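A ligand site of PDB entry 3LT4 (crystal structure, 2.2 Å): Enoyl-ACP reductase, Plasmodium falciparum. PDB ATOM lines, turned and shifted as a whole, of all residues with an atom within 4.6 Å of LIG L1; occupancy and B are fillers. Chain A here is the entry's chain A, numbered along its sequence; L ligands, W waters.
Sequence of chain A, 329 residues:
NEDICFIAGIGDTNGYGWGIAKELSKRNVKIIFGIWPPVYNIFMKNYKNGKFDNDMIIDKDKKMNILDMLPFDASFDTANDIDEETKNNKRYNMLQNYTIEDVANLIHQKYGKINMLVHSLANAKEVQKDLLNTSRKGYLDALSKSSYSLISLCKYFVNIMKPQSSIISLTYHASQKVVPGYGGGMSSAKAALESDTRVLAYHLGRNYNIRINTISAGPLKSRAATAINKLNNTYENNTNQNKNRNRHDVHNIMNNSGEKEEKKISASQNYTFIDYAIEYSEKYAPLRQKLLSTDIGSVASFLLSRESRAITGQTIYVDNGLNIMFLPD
OG of Ser 75 sits at hydrogen-bond distance from N3 of LIG L1. An oxygen (O5) of LIG L1 is in hydrogen-bond range of the backbone NH (N) of Gly 11 (3.3 Å). The backbone carbonyl oxygen (O) of Leu 220 sits at hydrogen-bond distance from a nitrogen (N7) of LIG L1, at 3.1 Å. O12 of LIG L1 is in hydrogen-bond range of O of Leu 121. An oxygen (O9) of LIG L1 sits at hydrogen-bond distance from the backbone NH of Tyr 16 (2.9 Å). The backbone NH of Ala 74 is in hydrogen-bond range of a nitrogen (N4) of LIG L1 (2.8 Å). The side-chain amide oxygen (OD1) of Asn 123 sits close to a nitrogen (N2) of LIG L1 (3.2 Å). The side-chain hydroxyl (OG) of Ser 222 sits at hydrogen-bond distance from an oxygen (O8) of LIG L1 (2.9 Å). N of Ala 224 sits at hydrogen-bond distance from O1 of LIG L1 (3.2 Å). The guanidinium group of Arg 223 lies within salt-bridge range of an oxygen (O1) of LIG L1. The side-chain carboxylate (OD1) of Asp 73 is in hydrogen-bond range of a nitrogen (N3) of LIG L1. The side-chain amino group (NZ) of Lys 190 lies within hydrogen-bond range of an oxygen (O13) of LIG L1. N of Leu 220 sits at hydrogen-bond distance from O14 of LIG L1. The side-chain hydroxyl (OH) of Tyr 182 sits at hydrogen-bond distance from an oxygen (O2) of LG2 L2.
O2 of LG2 L2 sits at hydrogen-bond distance from O13 of LIG L1, 2.6 Å away.
N of Gly 17 sits at hydrogen-bond distance from OG of Ser 120 (3.4 Å). OH of Tyr 16 sits at hydrogen-bond distance from O of Gly 218 (2.6 Å). N of Ala 225 lies within hydrogen-bond range of OG of Ser 222 (3.1 Å). The side-chain amino group of Lys 145 lies close to the side-chain hydroxyl of Ser 75 (3.3 Å). The backbone carbonyl oxygen (O) of Leu 170 lies within hydrogen-bond range of the side-chain amino group (NZ) of Lys 190 (2.8 Å). N of Ala 217 is in hydrogen-bond range of O of Thr 171, at 3.3 Å. The side-chain carboxylate (OD1) of Asp 73 is in hydrogen-bond range of the side-chain hydroxyl (OG) of Ser 75 (2.9 Å).
The indole nitrogen (NE1) of Trp 36 sits close to a nitrogen (N3) of LIG L1 (3.4 Å). Residues that only touch LIG L1: Gly 9, Ile 10, Gly 15, Phe 72, Ser 120, Ala 122, Leu 170, Thr 171, Tyr 172, Ala 217, Gly 218, Pro 219 and Ile 274. Of the 32 residues printed, 26 come within 4 Å of LIG L1.
Water W6 lies within hydrogen-bond range of an oxygen (O2) of LIG L1, the backbone NH of Gly 11 and the side-chain carboxylate of Asp 12. Water W3 lies within hydrogen-bond range of the side-chain carboxylate of Asp 12, the backbone NH of Arg 223, an oxygen (O2) of LIG L1 and the backbone NH of Gly 15. Water W7 lies within hydrogen-bond range of N of Gly 17 (2.9 Å), O of Gly 9 (2.9 Å), O9 of LIG L1 (3.0 Å) and OG of Ser 120 (3.1 Å). Water W5 lies within hydrogen-bond range of the backbone carbonyl oxygen (O) of Ile 10 (2.5 Å), the backbone NH (N) of Trp 36 (3.1 Å) and an oxygen (O6) of LIG L1 (3.1 Å). Water W4 lies within hydrogen-bond range of O of Leu 170, O12 of LIG L1 and O of Leu 121. Water W8 lies within hydrogen-bond range of the side-chain amino group of Lys 145 (2.9 Å), a nitrogen (N3) of LIG L1 (3.3 Å) and the side-chain amide oxygen of Asn 123 (3.4 Å).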
ATOM      1  N   GLY A   9      -2.701  10.251  -5.247  1.00  0.00           N
ATOM      2  CA  GLY A   9      -1.854  11.397  -5.550  1.00  0.00           C
ATOM      3  C   GLY A   9      -1.461  11.545  -7.006  1.00  0.00           C
ATOM      4  O   GLY A   9      -0.306  11.754  -7.300  1.00  0.00           O
ATOM      5  N   ILE A  10      -2.406  11.405  -7.920  1.00  0.00           N
ATOM      6  CA  ILE A  10      -2.152  11.673  -9.338  1.00  0.00           C
ATOM      7  C   ILE A  10      -2.929  12.943  -9.715  1.00  0.00           C
ATOM      8  O   ILE A  10      -4.123  13.050  -9.416  1.00  0.00           O
ATOM      9  CB  ILE A  10      -2.534  10.458 -10.218  1.00  0.00           C
ATOM     10  CG1 ILE A  10      -1.493   9.353 -10.016  1.00  0.00           C
ATOM     11  CG2 ILE A  10      -2.575  10.844 -11.720  1.00  0.00           C
ATOM     12  CD1 ILE A  10      -1.787   8.024 -10.684  1.00  0.00           C
ATOM     13  N   GLY A  11      -2.231  13.934 -10.289  1.00  0.00           N
ATOM     14  CA  GLY A  11      -2.818  15.205 -10.715  1.00  0.00           C
ATOM     15  C   GLY A  11      -2.650  15.500 -12.198  1.00  0.00           C
ATOM     16  O   GLY A  11      -3.346  16.360 -12.764  1.00  0.00           O
ATOM     17  N   ASP A  12      -1.737  14.766 -12.835  1.00  0.00           N
ATOM     18  CA  ASP A  12      -1.402  14.924 -14.232  1.00  0.00           C
ATOM     19  C   ASP A  12      -0.410  13.793 -14.534  1.00  0.00           C
ATOM     20  O   ASP A  12      -0.236  12.874 -13.725  1.00  0.00           O
ATOM     21  CB  ASP A  12      -0.739  16.279 -14.438  1.00  0.00           C
ATOM     22  CG  ASP A  12       0.509  16.466 -13.566  1.00  0.00           C
ATOM     23  OD1 ASP A  12       0.643  17.526 -12.958  1.00  0.00           O
ATOM     24  OD2 ASP A  12       1.368  15.554 -13.479  1.00  0.00           O
ATOM     25  N   GLY A  15       4.202  13.569 -12.677  1.00  0.00           N
ATOM     26  CA  GLY A  15       4.778  13.241 -11.379  1.00  0.00           C
ATOM     27  C   GLY A  15       5.083  11.757 -11.266  1.00  0.00           C
ATOM     28  O   GLY A  15       4.932  11.005 -12.228  1.00  0.00           O
ATOM     29  N   TYR A  16       5.451  11.342 -10.054  1.00  0.00           N
ATOM     30  CA  TYR A  16       5.822   9.958  -9.813  1.00  0.00           C
ATOM     31  C   TYR A  16       4.619   9.013  -9.787  1.00  0.00           C
ATOM     32  O   TYR A  16       4.745   7.847 -10.130  1.00  0.00           O
ATOM     33  CB  TYR A  16       6.643   9.842  -8.533  1.00  0.00           C
ATOM     34  CG  TYR A  16       8.120  10.221  -8.699  1.00  0.00           C
ATOM     35  CD1 TYR A  16       8.886   9.628  -9.686  1.00  0.00           C
ATOM     36  CD2 TYR A  16       8.734  11.147  -7.848  1.00  0.00           C
ATOM     37  CE1 TYR A  16      10.216   9.940  -9.855  1.00  0.00           C
ATOM     38  CE2 TYR A  16      10.078  11.465  -8.001  1.00  0.00           C
ATOM     39  CZ  TYR A  16      10.814  10.839  -9.004  1.00  0.00           C
ATOM     40  OH  TYR A  16      12.143  11.093  -9.213  1.00  0.00           O
ATOM     41  N   GLY A  17       3.447   9.508  -9.390  1.00  0.00           N
ATOM     42  CA  GLY A  17       2.233   8.670  -9.406  1.00  0.00           C
ATOM     43  C   GLY A  17       1.959   8.061 -10.769  1.00  0.00           C
ATOM     44  O   GLY A  17       1.679   6.858 -10.901  1.00  0.00           O
ATOM     45  N   TRP A  36      -6.807  14.536  -5.988  1.00  0.00           N
ATOM     46  CA  TRP A  36      -7.118  15.659  -5.115  1.00  0.00           C
ATOM     47  C   TRP A  36      -8.278  16.493  -5.733  1.00  0.00           C
ATOM     48  O   TRP A  36      -8.212  16.882  -6.893  1.00  0.00           O
ATOM     49  CB  TRP A  36      -5.872  16.497  -4.926  1.00  0.00           C
ATOM     50  CG  TRP A  36      -5.927  17.470  -3.800  1.00  0.00           C
ATOM     51  CD1 TRP A  36      -6.478  17.264  -2.570  1.00  0.00           C
ATOM     52  CD2 TRP A  36      -5.351  18.774  -3.774  1.00  0.00           C
ATOM     53  NE1 TRP A  36      -6.334  18.391  -1.799  1.00  0.00           N
ATOM     54  CE2 TRP A  36      -5.625  19.326  -2.504  1.00  0.00           C
ATOM     55  CE3 TRP A  36      -4.653  19.538  -4.716  1.00  0.00           C
ATOM     56  CZ2 TRP A  36      -5.212  20.612  -2.133  1.00  0.00           C
ATOM     57  CZ3 TRP A  36      -4.245  20.831  -4.355  1.00  0.00           C
ATOM     58  CH2 TRP A  36      -4.538  21.348  -3.071  1.00  0.00           C
ATOM     59  N   VAL A  39      -8.275  19.498  -8.252  1.00  0.00           N
ATOM     60  CA  VAL A  39      -7.817  19.233  -9.624  1.00  0.00           C
ATOM     61  C   VAL A  39      -8.566  18.077 -10.294  1.00  0.00           C
ATOM     62  O   VAL A  39      -8.250  17.694 -11.423  1.00  0.00           O
ATOM     63  CB  VAL A  39      -6.258  19.024  -9.725  1.00  0.00           C
ATOM     64  CG1 VAL A  39      -5.496  20.094  -8.933  1.00  0.00           C
ATOM     65  CG2 VAL A  39      -5.841  17.616  -9.290  1.00  0.00           C
ATOM     66  N   PHE A  72     -10.141  12.219  -4.022  1.00  0.00           N
ATOM     67  CA  PHE A  72      -9.517  11.728  -2.798  1.00  0.00           C
ATOM     68  C   PHE A  72      -8.774  12.879  -2.146  1.00  0.00           C
ATOM     69  O   PHE A  72      -7.920  13.501  -2.772  1.00  0.00           O
ATOM     70  CB  PHE A  72      -8.519  10.604  -3.136  1.00  0.00           C
ATOM     71  CG  PHE A  72      -7.686  10.161  -1.967  1.00  0.00           C
ATOM     72  CD1 PHE A  72      -8.191   9.234  -1.039  1.00  0.00           C
ATOM     73  CD2 PHE A  72      -6.405  10.673  -1.770  1.00  0.00           C
ATOM     74  CE1 PHE A  72      -7.427   8.834   0.066  1.00  0.00           C
ATOM     75  CE2 PHE A  72      -5.646  10.304  -0.659  1.00  0.00           C
ATOM     76  CZ  PHE A  72      -6.148   9.387   0.256  1.00  0.00           C
ATOM     77  N   ASP A  73      -9.151  13.194  -0.907  1.00  0.00           N
ATOM     78  CA  ASP A  73      -8.473  14.244  -0.148  1.00  0.00           C
ATOM     79  C   ASP A  73      -7.919  13.689   1.166  1.00  0.00           C
ATOM     80  O   ASP A  73      -8.673  13.290   2.042  1.00  0.00           O
ATOM     81  CB  ASP A  73      -9.413  15.431   0.126  1.00  0.00           C
ATOM     82  CG  ASP A  73      -8.651  16.683   0.609  1.00  0.00           C
ATOM     83  OD1 ASP A  73      -7.543  16.524   1.186  1.00  0.00           O
ATOM     84  OD2 ASP A  73      -9.140  17.823   0.407  1.00  0.00           O
ATOM     85  N   ALA A  74      -6.581  13.702   1.278  1.00  0.00           N
ATOM     86  CA  ALA A  74      -5.824  13.102   2.398  1.00  0.00           C
ATOM     87  C   ALA A  74      -5.832  13.996   3.624  1.00  0.00           C
ATOM     88  O   ALA A  74      -5.223  13.684   4.641  1.00  0.00           O
ATOM     89  CB  ALA A  74      -4.395  12.818   1.958  1.00  0.00           C
ATOM     90  N   SER A  75      -6.500  15.144   3.510  1.00  0.00           N
ATOM     91  CA  SER A  75      -6.681  16.093   4.606  1.00  0.00           C
ATOM     92  C   SER A  75      -7.725  15.598   5.607  1.00  0.00           C
ATOM     93  O   SER A  75      -7.725  16.043   6.772  1.00  0.00           O
ATOM     94  CB  SER A  75      -7.194  17.426   4.068  1.00  0.00           C
ATOM     95  OG  SER A  75      -6.230  18.057   3.244  1.00  0.00           O
ATOM     96  N   SER A 120       1.426   8.708  -2.861  1.00  0.00           N
ATOM     97  CA  SER A 120       2.265   9.470  -3.750  1.00  0.00           C
ATOM     98  C   SER A 120       1.865  10.936  -3.689  1.00  0.00           C
ATOM     99  O   SER A 120       1.580  11.561  -4.707  1.00  0.00           O
ATOM    100  CB  SER A 120       2.146   8.921  -5.187  1.00  0.00           C
ATOM    101  OG  SER A 120       3.075   9.592  -6.019  1.00  0.00           O
ATOM    102  N   LEU A 121       1.781  11.465  -2.485  1.00  0.00           N
ATOM    103  CA  LEU A 121       1.231  12.787  -2.279  1.00  0.00           C
ATOM    104  C   LEU A 121       1.938  13.464  -1.122  1.00  0.00           C
ATOM    105  O   LEU A 121       2.486  12.801  -0.222  1.00  0.00           O
ATOM    106  CB  LEU A 121      -0.291  12.723  -2.010  1.00  0.00           C
ATOM    107  CG  LEU A 121      -0.771  12.075  -0.702  1.00  0.00           C
ATOM    108  CD1 LEU A 121      -0.883  13.142   0.400  1.00  0.00           C
ATOM    109  CD2 LEU A 121      -2.116  11.371  -0.911  1.00  0.00           C
ATOM    110  N   ALA A 122       1.903  14.797  -1.179  1.00  0.00           N
ATOM    111  CA  ALA A 122       2.452  15.641  -0.149  1.00  0.00           C
ATOM    112  C   ALA A 122       1.833  17.000  -0.305  1.00  0.00           C
ATOM    113  O   ALA A 122       1.409  17.393  -1.388  1.00  0.00           O
ATOM    114  CB  ALA A 122       4.006  15.716  -0.238  1.00  0.00           C
ATOM    115  N   ASN A 123       1.793  17.720   0.799  1.00  0.00           N
ATOM    116  CA  ASN A 123       1.429  19.122   0.766  1.00  0.00           C
ATOM    117  C   ASN A 123       1.978  19.802   2.005  1.00  0.00           C
ATOM    118  O   ASN A 123       2.221  19.156   3.041  1.00  0.00           O
ATOM    119  CB  ASN A 123      -0.110  19.328   0.626  1.00  0.00           C
ATOM    120  CG  ASN A 123      -0.457  20.503  -0.315  1.00  0.00           C
ATOM    121  OD1 ASN A 123      -1.516  20.510  -0.959  1.00  0.00           O
ATOM    122  ND2 ASN A 123       0.454  21.487  -0.387  1.00  0.00           N
ATOM    123  N   LYS A 145      -0.680  16.495   6.033  1.00  0.00           N
ATOM    124  CA  LYS A 145      -0.943  16.138   4.641  1.00  0.00           C
ATOM    125  C   LYS A 145       0.065  15.140   4.099  1.00  0.00           C
ATOM    126  O   LYS A 145      -0.298  14.288   3.292  1.00  0.00           O
ATOM    127  CB  LYS A 145      -0.944  17.377   3.759  1.00  0.00           C
ATOM    128  CG  LYS A 145      -1.910  18.485   4.230  1.00  0.00           C
ATOM    129  CD  LYS A 145      -3.324  18.007   4.463  1.00  0.00           C
ATOM    130  CE  LYS A 145      -4.138  19.127   5.141  1.00  0.00           C
ATOM    131  NZ  LYS A 145      -4.160  20.416   4.297  1.00  0.00           N
ATOM    132  N   LEU A 170       6.404   7.776  -1.002  1.00  0.00           N
ATOM    133  CA  LEU A 170       7.569   8.447  -1.586  1.00  0.00           C
ATOM    134  C   LEU A 170       8.136   9.430  -0.584  1.00  0.00           C
ATOM    135  O   LEU A 170       7.394  10.195   0.035  1.00  0.00           O
ATOM    136  CB  LEU A 170       7.208   9.148  -2.898  1.00  0.00           C
ATOM    137  CG  LEU A 170       6.699   8.189  -4.022  1.00  0.00           C
ATOM    138  CD1 LEU A 170       6.226   8.943  -5.214  1.00  0.00           C
ATOM    139  CD2 LEU A 170       7.759   7.207  -4.476  1.00  0.00           C
ATOM    140  N   THR A 171       9.449   9.392  -0.399  1.00  0.00           N
ATOM    141  CA  THR A 171      10.099  10.354   0.486  1.00  0.00           C
ATOM    142  C   THR A 171      11.229  11.069  -0.248  1.00  0.00           C
ATOM    143  O   THR A 171      11.428  10.850  -1.453  1.00  0.00           O
ATOM    144  CB  THR A 171      10.571   9.657   1.805  1.00  0.00           C
ATOM    145  OG1 THR A 171      11.079  10.641   2.708  1.00  0.00           O
ATOM    146  CG2 THR A 171      11.677   8.617   1.520  1.00  0.00           C
ATOM    147  N   TYR A 172      11.994  11.867   0.477  1.00  0.00           N
ATOM    148  CA  TYR A 172      13.090  12.633  -0.108  1.00  0.00           C
ATOM    149  C   TYR A 172      14.188  12.807   0.944  1.00  0.00           C
ATOM    150  O   TYR A 172      13.903  12.936   2.152  1.00  0.00           O
ATOM    151  CB  TYR A 172      12.573  13.998  -0.631  1.00  0.00           C
ATOM    152  CG  TYR A 172      13.658  14.856  -1.297  1.00  0.00           C
ATOM    153  CD1 TYR A 172      14.386  14.374  -2.394  1.00  0.00           C
ATOM    154  CD2 TYR A 172      13.935  16.133  -0.828  1.00  0.00           C
ATOM    155  CE1 TYR A 172      15.371  15.135  -2.986  1.00  0.00           C
ATOM    156  CE2 TYR A 172      14.922  16.916  -1.425  1.00  0.00           C
ATOM    157  CZ  TYR A 172      15.639  16.403  -2.489  1.00  0.00           C
ATOM    158  OH  TYR A 172      16.623  17.176  -3.073  1.00  0.00           O
ATOM    159  N   TYR A 182      13.993  23.241   0.841  1.00  0.00           N
ATOM    160  CA  TYR A 182      12.909  22.252   1.065  1.00  0.00           C
ATOM    161  C   TYR A 182      12.244  22.646   2.387  1.00  0.00           C
ATOM    162  O   TYR A 182      12.526  22.047   3.443  1.00  0.00           O
ATOM    163  CB  TYR A 182      13.498  20.830   1.128  1.00  0.00           C
ATOM    164  CG  TYR A 182      12.505  19.685   0.897  1.00  0.00           C
ATOM    165  CD1 TYR A 182      11.909  19.484  -0.361  1.00  0.00           C
ATOM    166  CD2 TYR A 182      12.171  18.817   1.941  1.00  0.00           C
ATOM    167  CE1 TYR A 182      11.009  18.447  -0.560  1.00  0.00           C
ATOM    168  CE2 TYR A 182      11.280  17.763   1.754  1.00  0.00           C
ATOM    169  CZ  TYR A 182      10.708  17.571   0.508  1.00  0.00           C
ATOM    170  OH  TYR A 182       9.856  16.509   0.331  1.00  0.00           O
ATOM    171  N   LYS A 190       8.903  14.329   6.000  1.00  0.00           N
ATOM    172  CA  LYS A 190       9.622  13.198   5.387  1.00  0.00           C
ATOM    173  C   LYS A 190      10.401  12.381   6.410  1.00  0.00           C
ATOM    174  O   LYS A 190      10.459  11.162   6.316  1.00  0.00           O
ATOM    175  CB  LYS A 190      10.550  13.662   4.259  1.00  0.00           C
ATOM    176  CG  LYS A 190       9.835  14.206   3.008  1.00  0.00           C
ATOM    177  CD  LYS A 190       8.715  13.252   2.517  1.00  0.00           C
ATOM    178  CE  LYS A 190       8.188  13.745   1.144  1.00  0.00           C
ATOM    179  NZ  LYS A 190       7.030  12.922   0.613  1.00  0.00           N
ATOM    180  N   ALA A 217      13.085   9.074  -3.632  1.00  0.00           N
ATOM    181  CA  ALA A 217      13.273   9.415  -5.056  1.00  0.00           C
ATOM    182  C   ALA A 217      14.225  10.608  -5.253  1.00  0.00           C
ATOM    183  O   ALA A 217      14.272  11.521  -4.424  1.00  0.00           O
ATOM    184  CB  ALA A 217      11.937   9.727  -5.693  1.00  0.00           C
ATOM    185  N   GLY A 218      14.964  10.614  -6.357  1.00  0.00           N
ATOM    186  CA  GLY A 218      15.695  11.814  -6.785  1.00  0.00           C
ATOM    187  C   GLY A 218      14.762  12.832  -7.431  1.00  0.00           C
ATOM    188  O   GLY A 218      13.544  12.583  -7.537  1.00  0.00           O
ATOM    189  N   PRO A 219      15.309  13.969  -7.894  1.00  0.00           N
ATOM    190  CA  PRO A 219      14.448  15.076  -8.347  1.00  0.00           C
ATOM    191  C   PRO A 219      13.774  14.828  -9.698  1.00  0.00           C
ATOM    192  O   PRO A 219      14.384  14.257 -10.619  1.00  0.00           O
ATOM    193  CB  PRO A 219      15.390  16.259  -8.431  1.00  0.00           C
ATOM    194  CG  PRO A 219      16.801  15.638  -8.660  1.00  0.00           C
ATOM    195  CD  PRO A 219      16.730  14.177  -8.272  1.00  0.00           C
ATOM    196  N   LEU A 220      12.504  15.220  -9.783  1.00  0.00           N
ATOM    197  CA  LEU A 220      11.688  15.083 -10.996  1.00  0.00           C
ATOM    198  C   LEU A 220      10.912  16.375 -11.121  1.00  0.00           C
ATOM    199  O   LEU A 220      10.392  16.901 -10.110  1.00  0.00           O
ATOM    200  CB  LEU A 220      10.700  13.934 -10.863  1.00  0.00           C
ATOM    201  CG  LEU A 220       9.759  13.595 -12.023  1.00  0.00           C
ATOM    202  CD1 LEU A 220      10.518  12.995 -13.210  1.00  0.00           C
ATOM    203  CD2 LEU A 220       8.658  12.639 -11.587  1.00  0.00           C
ATOM    204  N   SER A 222       8.072  17.663 -11.494  1.00  0.00           N
ATOM    205  CA  SER A 222       6.659  17.458 -11.355  1.00  0.00           C
ATOM    206  C   SER A 222       6.013  18.832 -11.077  1.00  0.00           C
ATOM    207  O   SER A 222       6.713  19.816 -10.803  1.00  0.00           O
ATOM    208  CB  SER A 222       6.408  16.560 -10.170  1.00  0.00           C
ATOM    209  OG  SER A 222       6.711  17.242  -8.972  1.00  0.00           O
ATOM    210  N   ARG A 223       4.686  18.879 -11.088  1.00  0.00           N
ATOM    211  CA  ARG A 223       3.981  20.109 -10.716  1.00  0.00           C
ATOM    212  C   ARG A 223       4.299  20.573  -9.280  1.00  0.00           C
ATOM    213  O   ARG A 223       4.671  21.741  -9.073  1.00  0.00           O
ATOM    214  CB  ARG A 223       2.478  19.974 -10.972  1.00  0.00           C
ATOM    215  CG  ARG A 223       1.647  21.107 -10.389  1.00  0.00           C
ATOM    216  CD  ARG A 223       0.753  20.543  -9.302  1.00  0.00           C
ATOM    217  NE  ARG A 223       0.946  21.211  -8.023  1.00  0.00           N
ATOM    218  CZ  ARG A 223       0.883  20.582  -6.851  1.00  0.00           C
ATOM    219  NH1 ARG A 223       0.650  19.278  -6.814  1.00  0.00           N
ATOM    220  NH2 ARG A 223       1.074  21.251  -5.723  1.00  0.00           N
ATOM    221  N   ALA A 224       4.182  19.670  -8.297  1.00  0.00           N
ATOM    222  CA  ALA A 224       4.564  20.050  -6.927  1.00  0.00           C
ATOM    223  C   ALA A 224       6.003  20.598  -6.840  1.00  0.00           C
ATOM    224  O   ALA A 224       6.247  21.585  -6.166  1.00  0.00           O
ATOM    225  CB  ALA A 224       4.347  18.893  -5.951  1.00  0.00           C
ATOM    226  N   ALA A 225       6.954  19.962  -7.543  1.00  0.00           N
ATOM    227  CA  ALA A 225       8.350  20.369  -7.465  1.00  0.00           C
ATOM    228  C   ALA A 225       8.540  21.823  -7.952  1.00  0.00           C
ATOM    229  O   ALA A 225       9.294  22.590  -7.367  1.00  0.00           O
ATOM    230  CB  ALA A 225       9.208  19.444  -8.298  1.00  0.00           C
ATOM    231  N   ILE A 274      13.867  23.113  -8.157  1.00  0.00           N
ATOM    232  CA  ILE A 274      13.879  21.853  -8.872  1.00  0.00           C
ATOM    233  C   ILE A 274      14.871  21.846 -10.042  1.00  0.00           C
ATOM    234  O   ILE A 274      15.519  20.838 -10.264  1.00  0.00           O
ATOM    235  CB  ILE A 274      12.436  21.365  -9.304  1.00  0.00           C
ATOM    236  CG1 ILE A 274      12.441  19.857  -9.627  1.00  0.00           C
ATOM    237  CG2 ILE A 274      11.864  22.197 -10.471  1.00  0.00           C
ATOM    238  CD1 ILE A 274      12.832  18.980  -8.446  1.00  0.00           C
HETATM  239  P1  LIG L   1       2.914  15.723  -8.050  1.00  0.00           P
HETATM  240  O1  LIG L   1       2.296  17.096  -7.931  1.00  0.00           O
HETATM  241  O2  LIG L   1       2.890  14.967  -9.351  1.00  0.00           O
HETATM  242  O3  LIG L   1       2.272  14.768  -6.922  1.00  0.00           O
HETATM  243  C1  LIG L   1       1.687  15.327  -5.738  1.00  0.00           C
HETATM  244  C2  LIG L   1       0.180  15.121  -5.794  1.00  0.00           C
HETATM  245  O4  LIG L   1      -0.386  15.132  -4.481  1.00  0.00           O
HETATM  246  C3  LIG L   1      -0.522  16.213  -6.594  1.00  0.00           C
HETATM  247  O5  LIG L   1      -1.147  15.646  -7.748  1.00  0.00           O
HETATM  248  C4  LIG L   1      -1.578  16.770  -5.669  1.00  0.00           C
HETATM  249  O6  LIG L   1      -2.826  16.946  -6.345  1.00  0.00           O
HETATM  250  C5  LIG L   1      -1.692  15.700  -4.595  1.00  0.00           C
HETATM  251  N1  LIG L   1      -2.175  16.273  -3.306  1.00  0.00           N
HETATM  252  C6  LIG L   1      -1.791  17.410  -2.710  1.00  0.00           C
HETATM  253  N2  LIG L   1      -2.491  17.570  -1.560  1.00  0.00           N
HETATM  254  C7  LIG L   1      -3.312  16.513  -1.446  1.00  0.00           C
HETATM  255  C8  LIG L   1      -4.329  16.079  -0.447  1.00  0.00           C
HETATM  256  N3  LIG L   1      -4.577  16.809   0.667  1.00  0.00           N
HETATM  257  N4  LIG L   1      -4.987  14.924  -0.674  1.00  0.00           N
HETATM  258  C9  LIG L   1      -4.733  14.198  -1.769  1.00  0.00           C
HETATM  259  N5  LIG L   1      -3.835  14.574  -2.686  1.00  0.00           N
HETATM  260  C10 LIG L   1      -3.118  15.703  -2.557  1.00  0.00           C
HETATM  261  O7  LIG L   1       4.445  15.865  -7.568  1.00  0.00           O
HETATM  262  P2  LIG L   1       5.331  14.562  -7.218  1.00  0.00           P
HETATM  263  O8  LIG L   1       6.769  15.021  -7.080  1.00  0.00           O
HETATM  264  O9  LIG L   1       4.986  13.471  -8.203  1.00  0.00           O
HETATM  265  O10 LIG L   1       4.793  14.136  -5.760  1.00  0.00           O
HETATM  266  C11 LIG L   1       4.575  12.752  -5.473  1.00  0.00           C
HETATM  267  C12 LIG L   1       5.378  12.327  -4.256  1.00  0.00           C
HETATM  268  O11 LIG L   1       6.749  12.081  -4.590  1.00  0.00           O
HETATM  269  C13 LIG L   1       5.387  13.408  -3.175  1.00  0.00           C
HETATM  270  O12 LIG L   1       5.028  12.812  -1.917  1.00  0.00           O
HETATM  271  C14 LIG L   1       6.823  13.889  -3.115  1.00  0.00           C
HETATM  272  O13 LIG L   1       7.190  14.258  -1.791  1.00  0.00           O
HETATM  273  C15 LIG L   1       7.596  12.684  -3.611  1.00  0.00           C
HETATM  274  N6  LIG L   1       8.898  13.078  -4.144  1.00  0.00           N
HETATM  275  C16 LIG L   1       8.997  13.822  -5.256  1.00  0.00           C
HETATM  276  C17 LIG L   1      10.235  14.199  -5.765  1.00  0.00           C
HETATM  277  C18 LIG L   1      10.327  15.040  -7.005  1.00  0.00           C
HETATM  278  O14 LIG L   1      11.404  15.530  -7.307  1.00  0.00           O
HETATM  279  N7  LIG L   1       9.230  15.236  -7.734  1.00  0.00           N
HETATM  280  C19 LIG L   1      11.528  13.773  -5.089  1.00  0.00           C
HETATM  281  C20 LIG L   1      11.274  12.969  -3.904  1.00  0.00           C
HETATM  282  C21 LIG L   1       9.982  12.658  -3.489  1.00  0.00           C
HETATM  283  C1  LG2 L   2       8.619  17.041  -4.013  1.00  0.00           C
HETATM  284  C2  LG2 L   2       9.523  16.549  -3.071  1.00  0.00           C
HETATM  285  C3  LG2 L   2      10.888  16.631  -3.306  1.00  0.00           C
HETATM  286  C4  LG2 L   2      11.316  17.225  -4.499  1.00  0.00           C
HETATM  287  C5  LG2 L   2      10.412  17.718  -5.442  1.00  0.00           C
HETATM  288  C6  LG2 L   2       9.047  17.635  -5.206  1.00  0.00           C
HETATM  289  O1  LG2 L   2       7.287  16.952  -3.755  1.00  0.00           O
HETATM  290  C7  LG2 L   2       6.662  17.899  -2.990  1.00  0.00           C
HETATM  291  C8  LG2 L   2       5.283  17.844  -2.917  1.00  0.00           C
HETATM  292  C9  LG2 L   2       4.634  18.813  -2.171  1.00  0.00           C
HETATM  293  C10 LG2 L   2       5.373  19.804  -1.525  1.00  0.00           C
HETATM  294  C11 LG2 L   2       6.764  19.864  -1.591  1.00  0.00           C
HETATM  295  C12 LG2 L   2       7.416  18.904  -2.351  1.00  0.00           C
HETATM  296 CL1  LG2 L   2      13.080  17.310  -4.785  1.00  0.00          CL
HETATM  297 CL2  LG2 L   2       4.476  21.019  -0.563  1.00  0.00          CL
HETATM  298  N1  LG2 L   2       4.568  16.870  -3.575  1.00  0.00           N
HETATM  299  O2  LG2 L   2       9.092  16.015  -1.901  1.00  0.00           O
HETATM  300  O   HOH W   1      -0.023  17.276  -9.901  1.00  0.00           O
HETATM  301  O   HOH W   2      -2.050  18.532  -8.313  1.00  0.00           O
HETATM  302  O   HOH W   3       3.240  16.540 -11.698  1.00  0.00           O
HETATM  303  O   HOH W   4       4.468  10.040  -0.508  1.00  0.00           O
HETATM  304  O   HOH W   5      -4.044  14.289  -7.276  1.00  0.00           O
HETATM  305  O   HOH W   6       0.581  14.363 -10.706  1.00  0.00           O
HETATM  306  O   HOH W   7       2.478  11.846  -8.060  1.00  0.00           O
HETATM  307  O   HOH W   8      -3.788  19.883   1.457  1.00  0.00           O
